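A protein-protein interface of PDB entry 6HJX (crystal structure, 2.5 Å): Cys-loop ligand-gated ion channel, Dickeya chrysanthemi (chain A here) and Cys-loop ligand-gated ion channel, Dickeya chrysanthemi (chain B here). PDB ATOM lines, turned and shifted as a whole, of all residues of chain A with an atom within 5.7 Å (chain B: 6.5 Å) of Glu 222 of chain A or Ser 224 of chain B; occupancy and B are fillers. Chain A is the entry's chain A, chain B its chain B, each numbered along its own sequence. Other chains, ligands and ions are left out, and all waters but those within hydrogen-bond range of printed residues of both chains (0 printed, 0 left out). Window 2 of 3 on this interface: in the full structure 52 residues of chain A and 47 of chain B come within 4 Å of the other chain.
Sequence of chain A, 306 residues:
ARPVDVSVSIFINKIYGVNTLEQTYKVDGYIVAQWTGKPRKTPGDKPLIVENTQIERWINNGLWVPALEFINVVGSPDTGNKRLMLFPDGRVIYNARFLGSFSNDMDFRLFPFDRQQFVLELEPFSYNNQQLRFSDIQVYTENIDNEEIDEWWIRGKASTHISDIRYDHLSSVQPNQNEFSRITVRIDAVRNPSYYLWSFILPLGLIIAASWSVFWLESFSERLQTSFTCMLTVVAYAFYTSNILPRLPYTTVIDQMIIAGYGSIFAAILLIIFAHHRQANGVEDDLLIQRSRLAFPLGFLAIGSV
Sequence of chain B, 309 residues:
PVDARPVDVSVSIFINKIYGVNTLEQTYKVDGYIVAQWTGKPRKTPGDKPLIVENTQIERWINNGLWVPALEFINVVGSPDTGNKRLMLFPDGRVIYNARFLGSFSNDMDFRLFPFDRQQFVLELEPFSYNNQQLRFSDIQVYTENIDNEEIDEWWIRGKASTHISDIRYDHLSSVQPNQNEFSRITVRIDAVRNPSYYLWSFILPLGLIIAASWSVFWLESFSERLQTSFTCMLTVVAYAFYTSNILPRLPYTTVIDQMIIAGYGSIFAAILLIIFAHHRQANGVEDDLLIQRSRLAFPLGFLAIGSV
The side-chain hydroxyl (OG) of Ser 224 of chain B sits at hydrogen-bond distance from the side-chain carboxylate (OE2) of Glu 222 of chain A (2.8 Å). The side-chain hydroxyl (OG1) of Thr 226 of chain A sits at hydrogen-bond distance from the side-chain amide nitrogen (NE2) of Gln 228 of chain B, 3.2 Å away. OE2 of Glu 218 of chain A lies within hydrogen-bond range of NE2 of His 279 of chain B, 2.6 Å away.
N of Ser 219 of chain A sits close to OE1 of Glu 222 of chain A (3.4 Å). The side-chain hydroxyl of Ser 224 of chain B lies within hydrogen-bond range of the side-chain amide oxygen of Gln 228 of chain B, at 3.2 Å. The guanidinium group (NH1) of Arg 223 of chain A lies close to the backbone carbonyl oxygen (O) of Glu 218 of chain A (3.4 Å). The backbone carbonyl oxygen (O) of Glu 222 of chain A is in hydrogen-bond range of the side-chain hydroxyl (OG1) of Thr 226 of chain A, 2.9 Å away. The backbone carbonyl oxygen (O) of Leu 217 of chain A lies within hydrogen-bond range of the guanidinium group (NH1) of Arg 223 of chain A (3.1 Å).
Among the printed residues, pairs that only touch across the chains: Leu 217 of chain A with Leu 227 of chain B (3.7 Å).
Of the printed residues of chain B, Leu 217 of chain A touches Leu 227. Of the printed residues of chain B, Glu 218 of chain A touches His 279. Glu 222 of chain A touches just one residue of chain B: Ser 224. Arg 223 of chain A touches none of the printed residues of chain B. Of the printed residues of chain B, Thr 226 of chain A touches Gln 228 (3.2 Å). Of chain A, only Glu 222 (2.8 Å) comes within 4 Å of Ser 224 of chain B. Printed residues of chain A within 4 Å of Gln 228 of chain B: Thr 226. Ile 275 of chain B touches none of the printed residues of chain A. Of the printed residues of chain A, His 279 of chain B touches Glu 218 (2.6 Å). The nearest printed residue of chain B that does not touch Leu 217 of chain A is Phe 223 of chain B (4.1 Å).
Hydrophobic or aromatic side chains of chain B that line the printed part of chain A: Leu 227 and His 279. Printed residues of chain A that touch a printed residue of chain B: Leu 217, Glu 218, Glu 222 and Thr 226. Hydrophobic or aromatic side chains of chain A that line the printed part of chain B: Leu 217. Among the printed residues, no Asp or Glu carboxylate lies within 4 Å of a Lys or Arg side-chain nitrogen of the other chain.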
ATOM      1  N   LEU A 217     -14.236   5.886  26.245  1.00  0.00           N
ATOM      2  CA  LEU A 217     -15.516   6.410  25.792  1.00  0.00           C
ATOM      3  C   LEU A 217     -16.301   6.932  26.989  1.00  0.00           C
ATOM      4  O   LEU A 217     -16.154   6.450  28.117  1.00  0.00           O
ATOM      5  CB  LEU A 217     -16.315   5.329  25.063  1.00  0.00           C
ATOM      6  CG  LEU A 217     -15.825   4.933  23.669  1.00  0.00           C
ATOM      7  CD1 LEU A 217     -16.455   3.619  23.234  1.00  0.00           C
ATOM      8  CD2 LEU A 217     -16.132   6.028  22.657  1.00  0.00           C
ATOM      9  N   GLU A 218     -17.148   7.928  26.737  1.00  0.00           N
ATOM     10  CA  GLU A 218     -17.775   8.686  27.808  1.00  0.00           C
ATOM     11  C   GLU A 218     -19.261   8.404  27.979  1.00  0.00           C
ATOM     12  O   GLU A 218     -19.851   8.874  28.959  1.00  0.00           O
ATOM     13  CB  GLU A 218     -17.554  10.186  27.568  1.00  0.00           C
ATOM     14  CG  GLU A 218     -16.099  10.594  27.753  1.00  0.00           C
ATOM     15  CD  GLU A 218     -15.736  11.870  27.021  1.00  0.00           C
ATOM     16  OE1 GLU A 218     -16.607  12.437  26.328  1.00  0.00           O
ATOM     17  OE2 GLU A 218     -14.571  12.304  27.137  1.00  0.00           O
ATOM     18  N   SER A 219     -19.876   7.649  27.075  1.00  0.00           N
ATOM     19  CA  SER A 219     -21.268   7.241  27.204  1.00  0.00           C
ATOM     20  C   SER A 219     -21.343   5.746  27.477  1.00  0.00           C
ATOM     21  O   SER A 219     -20.596   4.961  26.886  1.00  0.00           O
ATOM     22  CB  SER A 219     -22.061   7.571  25.937  1.00  0.00           C
ATOM     23  OG  SER A 219     -23.366   7.024  26.004  1.00  0.00           O
ATOM     24  N   PHE A 220     -22.252   5.357  28.374  1.00  0.00           N
ATOM     25  CA  PHE A 220     -22.458   3.939  28.651  1.00  0.00           C
ATOM     26  C   PHE A 220     -22.839   3.183  27.385  1.00  0.00           C
ATOM     27  O   PHE A 220     -22.326   2.087  27.128  1.00  0.00           O
ATOM     28  CB  PHE A 220     -23.535   3.763  29.721  1.00  0.00           C
ATOM     29  CG  PHE A 220     -24.198   2.416  29.704  1.00  0.00           C
ATOM     30  CD1 PHE A 220     -23.532   1.295  30.165  1.00  0.00           C
ATOM     31  CD2 PHE A 220     -25.491   2.273  29.232  1.00  0.00           C
ATOM     32  CE1 PHE A 220     -24.144   0.054  30.150  1.00  0.00           C
ATOM     33  CE2 PHE A 220     -26.106   1.035  29.217  1.00  0.00           C
ATOM     34  CZ  PHE A 220     -25.434  -0.072  29.676  1.00  0.00           C
ATOM     35  N   SER A 221     -23.735   3.754  26.576  1.00  0.00           N
ATOM     36  CA  SER A 221     -24.146   3.089  25.345  1.00  0.00           C
ATOM     37  C   SER A 221     -22.969   2.919  24.391  1.00  0.00           C
ATOM     38  O   SER A 221     -22.805   1.859  23.778  1.00  0.00           O
ATOM     39  CB  SER A 221     -25.273   3.876  24.676  1.00  0.00           C
ATOM     40  OG  SER A 221     -25.752   3.196  23.530  1.00  0.00           O
ATOM     41  N   GLU A 222     -22.138   3.956  24.253  1.00  0.00           N
ATOM     42  CA  GLU A 222     -20.963   3.851  23.396  1.00  0.00           C
ATOM     43  C   GLU A 222     -20.002   2.787  23.910  1.00  0.00           C
ATOM     44  O   GLU A 222     -19.470   1.988  23.131  1.00  0.00           O
ATOM     45  CB  GLU A 222     -20.258   5.205  23.304  1.00  0.00           C
ATOM     46  CG  GLU A 222     -21.089   6.304  22.652  1.00  0.00           C
ATOM     47  CD  GLU A 222     -20.498   7.689  22.861  1.00  0.00           C
ATOM     48  OE1 GLU A 222     -19.566   7.827  23.684  1.00  0.00           O
ATOM     49  OE2 GLU A 222     -20.968   8.643  22.206  1.00  0.00           O
ATOM     50  N   ARG A 223     -19.774   2.755  25.226  1.00  0.00           N
ATOM     51  CA  ARG A 223     -18.831   1.800  25.796  1.00  0.00           C
ATOM     52  C   ARG A 223     -19.276   0.363  25.549  1.00  0.00           C
ATOM     53  O   ARG A 223     -18.453  -0.502  25.221  1.00  0.00           O
ATOM     54  CB  ARG A 223     -18.671   2.054  27.296  1.00  0.00           C
ATOM     55  CG  ARG A 223     -17.895   3.311  27.644  1.00  0.00           C
ATOM     56  CD  ARG A 223     -17.624   3.402  29.140  1.00  0.00           C
ATOM     57  NE  ARG A 223     -18.842   3.626  29.916  1.00  0.00           N
ATOM     58  CZ  ARG A 223     -19.283   4.820  30.305  1.00  0.00           C
ATOM     59  NH1 ARG A 223     -18.614   5.925  29.998  1.00  0.00           N
ATOM     60  NH2 ARG A 223     -20.403   4.908  31.007  1.00  0.00           N
ATOM     61  N   LEU A 224     -20.574   0.088  25.693  1.00  0.00           N
ATOM     62  CA  LEU A 224     -21.060  -1.286  25.624  1.00  0.00           C
ATOM     63  C   LEU A 224     -21.140  -1.783  24.186  1.00  0.00           C
ATOM     64  O   LEU A 224     -20.723  -2.910  23.889  1.00  0.00           O
ATOM     65  CB  LEU A 224     -22.427  -1.384  26.303  1.00  0.00           C
ATOM     66  CG  LEU A 224     -23.101  -2.758  26.288  1.00  0.00           C
ATOM     67  CD1 LEU A 224     -22.196  -3.833  26.873  1.00  0.00           C
ATOM     68  CD2 LEU A 224     -24.412  -2.707  27.048  1.00  0.00           C
ATOM     69  N   GLN A 225     -21.671  -0.963  23.278  1.00  0.00           N
ATOM     70  CA  GLN A 225     -21.808  -1.393  21.891  1.00  0.00           C
ATOM     71  C   GLN A 225     -20.447  -1.582  21.231  1.00  0.00           C
ATOM     72  O   GLN A 225     -20.240  -2.551  20.492  1.00  0.00           O
ATOM     73  CB  GLN A 225     -22.652  -0.383  21.113  1.00  0.00           C
ATOM     74  CG  GLN A 225     -24.117  -0.356  21.541  1.00  0.00           C
ATOM     75  CD  GLN A 225     -24.932   0.681  20.789  1.00  0.00           C
ATOM     76  OE1 GLN A 225     -24.561   1.853  20.726  1.00  0.00           O
ATOM     77  NE2 GLN A 225     -26.047   0.251  20.210  1.00  0.00           N
ATOM     78  N   THR A 226     -19.506  -0.670  21.486  1.00  0.00           N
ATOM     79  CA  THR A 226     -18.167  -0.819  20.926  1.00  0.00           C
ATOM     80  C   THR A 226     -17.531  -2.137  21.347  1.00  0.00           C
ATOM     81  O   THR A 226     -16.762  -2.728  20.579  1.00  0.00           O
ATOM     82  CB  THR A 226     -17.286   0.355  21.355  1.00  0.00           C
ATOM     83  OG1 THR A 226     -17.822   1.573  20.823  1.00  0.00           O
ATOM     84  CG2 THR A 226     -15.852   0.171  20.863  1.00  0.00           C
ATOM     85  N   SER A 227     -17.833  -2.611  22.558  1.00  0.00           N
ATOM     86  CA  SER A 227     -17.277  -3.880  23.012  1.00  0.00           C
ATOM     87  C   SER A 227     -17.754  -5.037  22.147  1.00  0.00           C
ATOM     88  O   SER A 227     -17.024  -6.018  21.969  1.00  0.00           O
ATOM     89  CB  SER A 227     -17.647  -4.123  24.475  1.00  0.00           C
ATOM     90  OG  SER A 227     -16.908  -3.270  25.331  1.00  0.00           O
ATOM     91  N   SER B 222     -16.938  14.292  15.801  1.00  0.00           N
ATOM     92  CA  SER B 222     -16.925  13.981  17.223  1.00  0.00           C
ATOM     93  C   SER B 222     -15.907  12.888  17.526  1.00  0.00           C
ATOM     94  O   SER B 222     -15.669  11.990  16.714  1.00  0.00           O
ATOM     95  CB  SER B 222     -18.309  13.533  17.701  1.00  0.00           C
ATOM     96  OG  SER B 222     -18.611  12.232  17.230  1.00  0.00           O
ATOM     97  N   PHE B 223     -15.309  12.979  18.717  1.00  0.00           N
ATOM     98  CA  PHE B 223     -14.387  11.946  19.179  1.00  0.00           C
ATOM     99  C   PHE B 223     -15.044  10.571  19.143  1.00  0.00           C
ATOM    100  O   PHE B 223     -14.449   9.597  18.666  1.00  0.00           O
ATOM    101  CB  PHE B 223     -13.909  12.289  20.593  1.00  0.00           C
ATOM    102  CG  PHE B 223     -13.408  11.107  21.375  1.00  0.00           C
ATOM    103  CD1 PHE B 223     -12.112  10.645  21.208  1.00  0.00           C
ATOM    104  CD2 PHE B 223     -14.229  10.470  22.291  1.00  0.00           C
ATOM    105  CE1 PHE B 223     -11.651   9.561  21.935  1.00  0.00           C
ATOM    106  CE2 PHE B 223     -13.772   9.389  23.019  1.00  0.00           C
ATOM    107  CZ  PHE B 223     -12.481   8.934  22.841  1.00  0.00           C
ATOM    108  N   SER B 224     -16.279  10.475  19.638  1.00  0.00           N
ATOM    109  CA  SER B 224     -16.977   9.194  19.641  1.00  0.00           C
ATOM    110  C   SER B 224     -17.100   8.616  18.238  1.00  0.00           C
ATOM    111  O   SER B 224     -17.077   7.392  18.069  1.00  0.00           O
ATOM    112  CB  SER B 224     -18.364   9.354  20.266  1.00  0.00           C
ATOM    113  OG  SER B 224     -19.074   8.129  20.240  1.00  0.00           O
ATOM    114  N   GLU B 225     -17.238   9.472  17.221  1.00  0.00           N
ATOM    115  CA  GLU B 225     -17.342   8.983  15.851  1.00  0.00           C
ATOM    116  C   GLU B 225     -15.996   8.489  15.334  1.00  0.00           C
ATOM    117  O   GLU B 225     -15.930   7.484  14.618  1.00  0.00           O
ATOM    118  CB  GLU B 225     -17.884  10.084  14.940  1.00  0.00           C
ATOM    119  CG  GLU B 225     -19.379  10.317  15.069  1.00  0.00           C
ATOM    120  CD  GLU B 225     -19.839  11.559  14.328  1.00  0.00           C
ATOM    121  OE1 GLU B 225     -19.071  12.543  14.271  1.00  0.00           O
ATOM    122  OE2 GLU B 225     -20.967  11.548  13.797  1.00  0.00           O
ATOM    123  N   ARG B 226     -14.912   9.185  15.683  1.00  0.00           N
ATOM    124  CA  ARG B 226     -13.596   8.800  15.189  1.00  0.00           C
ATOM    125  C   ARG B 226     -13.148   7.465  15.767  1.00  0.00           C
ATOM    126  O   ARG B 226     -12.454   6.699  15.088  1.00  0.00           O
ATOM    127  CB  ARG B 226     -12.576   9.893  15.515  1.00  0.00           C
ATOM    128  CG  ARG B 226     -12.910  11.232  14.876  1.00  0.00           C
ATOM    129  CD  ARG B 226     -11.778  12.240  14.990  1.00  0.00           C
ATOM    130  NE  ARG B 226     -11.691  12.830  16.324  1.00  0.00           N
ATOM    131  CZ  ARG B 226     -12.482  13.803  16.769  1.00  0.00           C
ATOM    132  NH1 ARG B 226     -13.438  14.302  15.994  1.00  0.00           N
ATOM    133  NH2 ARG B 226     -12.321  14.276  17.997  1.00  0.00           N
ATOM    134  N   LEU B 227     -13.545   7.160  17.003  1.00  0.00           N
ATOM    135  CA  LEU B 227     -13.084   5.941  17.657  1.00  0.00           C
ATOM    136  C   LEU B 227     -13.860   4.722  17.170  1.00  0.00           C
ATOM    137  O   LEU B 227     -13.263   3.711  16.784  1.00  0.00           O
ATOM    138  CB  LEU B 227     -13.205   6.088  19.175  1.00  0.00           C
ATOM    139  CG  LEU B 227     -12.381   5.115  20.020  1.00  0.00           C
ATOM    140  CD1 LEU B 227     -10.888   5.368  19.846  1.00  0.00           C
ATOM    141  CD2 LEU B 227     -12.766   5.221  21.484  1.00  0.00           C
ATOM    142  N   GLN B 228     -15.194   4.800  17.173  1.00  0.00           N
ATOM    143  CA  GLN B 228     -16.001   3.653  16.774  1.00  0.00           C
ATOM    144  C   GLN B 228     -15.810   3.308  15.303  1.00  0.00           C
ATOM    145  O   GLN B 228     -15.929   2.137  14.923  1.00  0.00           O
ATOM    146  CB  GLN B 228     -17.475   3.923  17.073  1.00  0.00           C
ATOM    147  CG  GLN B 228     -17.791   4.050  18.559  1.00  0.00           C
ATOM    148  CD  GLN B 228     -19.244   4.403  18.819  1.00  0.00           C
ATOM    149  OE1 GLN B 228     -19.688   5.511  18.519  1.00  0.00           O
ATOM    150  NE2 GLN B 228     -19.992   3.456  19.373  1.00  0.00           N
ATOM    151  N   THR B 229     -15.512   4.301  14.461  1.00  0.00           N
ATOM    152  CA  THR B 229     -15.299   4.023  13.045  1.00  0.00           C
ATOM    153  C   THR B 229     -13.963   3.325  12.817  1.00  0.00           C
ATOM    154  O   THR B 229     -13.850   2.462  11.939  1.00  0.00           O
ATOM    155  CB  THR B 229     -15.375   5.320  12.235  1.00  0.00           C
ATOM    156  OG1 THR B 229     -16.700   5.861  12.323  1.00  0.00           O
ATOM    157  CG2 THR B 229     -15.030   5.072  10.766  1.00  0.00           C
ATOM    158  N   ILE B 275      -6.482   9.702  18.301  1.00  0.00           N
ATOM    159  CA  ILE B 275      -7.847  10.147  18.575  1.00  0.00           C
ATOM    160  C   ILE B 275      -8.064  10.287  20.077  1.00  0.00           C
ATOM    161  O   ILE B 275      -8.555  11.315  20.557  1.00  0.00           O
ATOM    162  CB  ILE B 275      -8.858   9.173  17.942  1.00  0.00           C
ATOM    163  CG1 ILE B 275      -8.751   9.222  16.415  1.00  0.00           C
ATOM    164  CG2 ILE B 275     -10.282   9.503  18.373  1.00  0.00           C
ATOM    165  CD1 ILE B 275      -9.318   8.001  15.720  1.00  0.00           C
ATOM    166  N   HIS B 279      -8.330  13.891  22.575  1.00  0.00           N
ATOM    167  CA  HIS B 279      -9.562  14.124  23.319  1.00  0.00           C
ATOM    168  C   HIS B 279      -9.362  14.115  24.830  1.00  0.00           C
ATOM    169  O   HIS B 279     -10.240  14.592  25.556  1.00  0.00           O
ATOM    170  CB  HIS B 279     -10.614  13.077  22.947  1.00  0.00           C
ATOM    171  CG  HIS B 279     -11.942  13.308  23.594  1.00  0.00           C
ATOM    172  ND1 HIS B 279     -12.897  14.143  23.053  1.00  0.00           N
ATOM    173  CD2 HIS B 279     -12.470  12.828  24.744  1.00  0.00           C
ATOM    174  CE1 HIS B 279     -13.960  14.159  23.838  1.00  0.00           C
ATOM    175  NE2 HIS B 279     -13.725  13.370  24.872  1.00  0.00           N
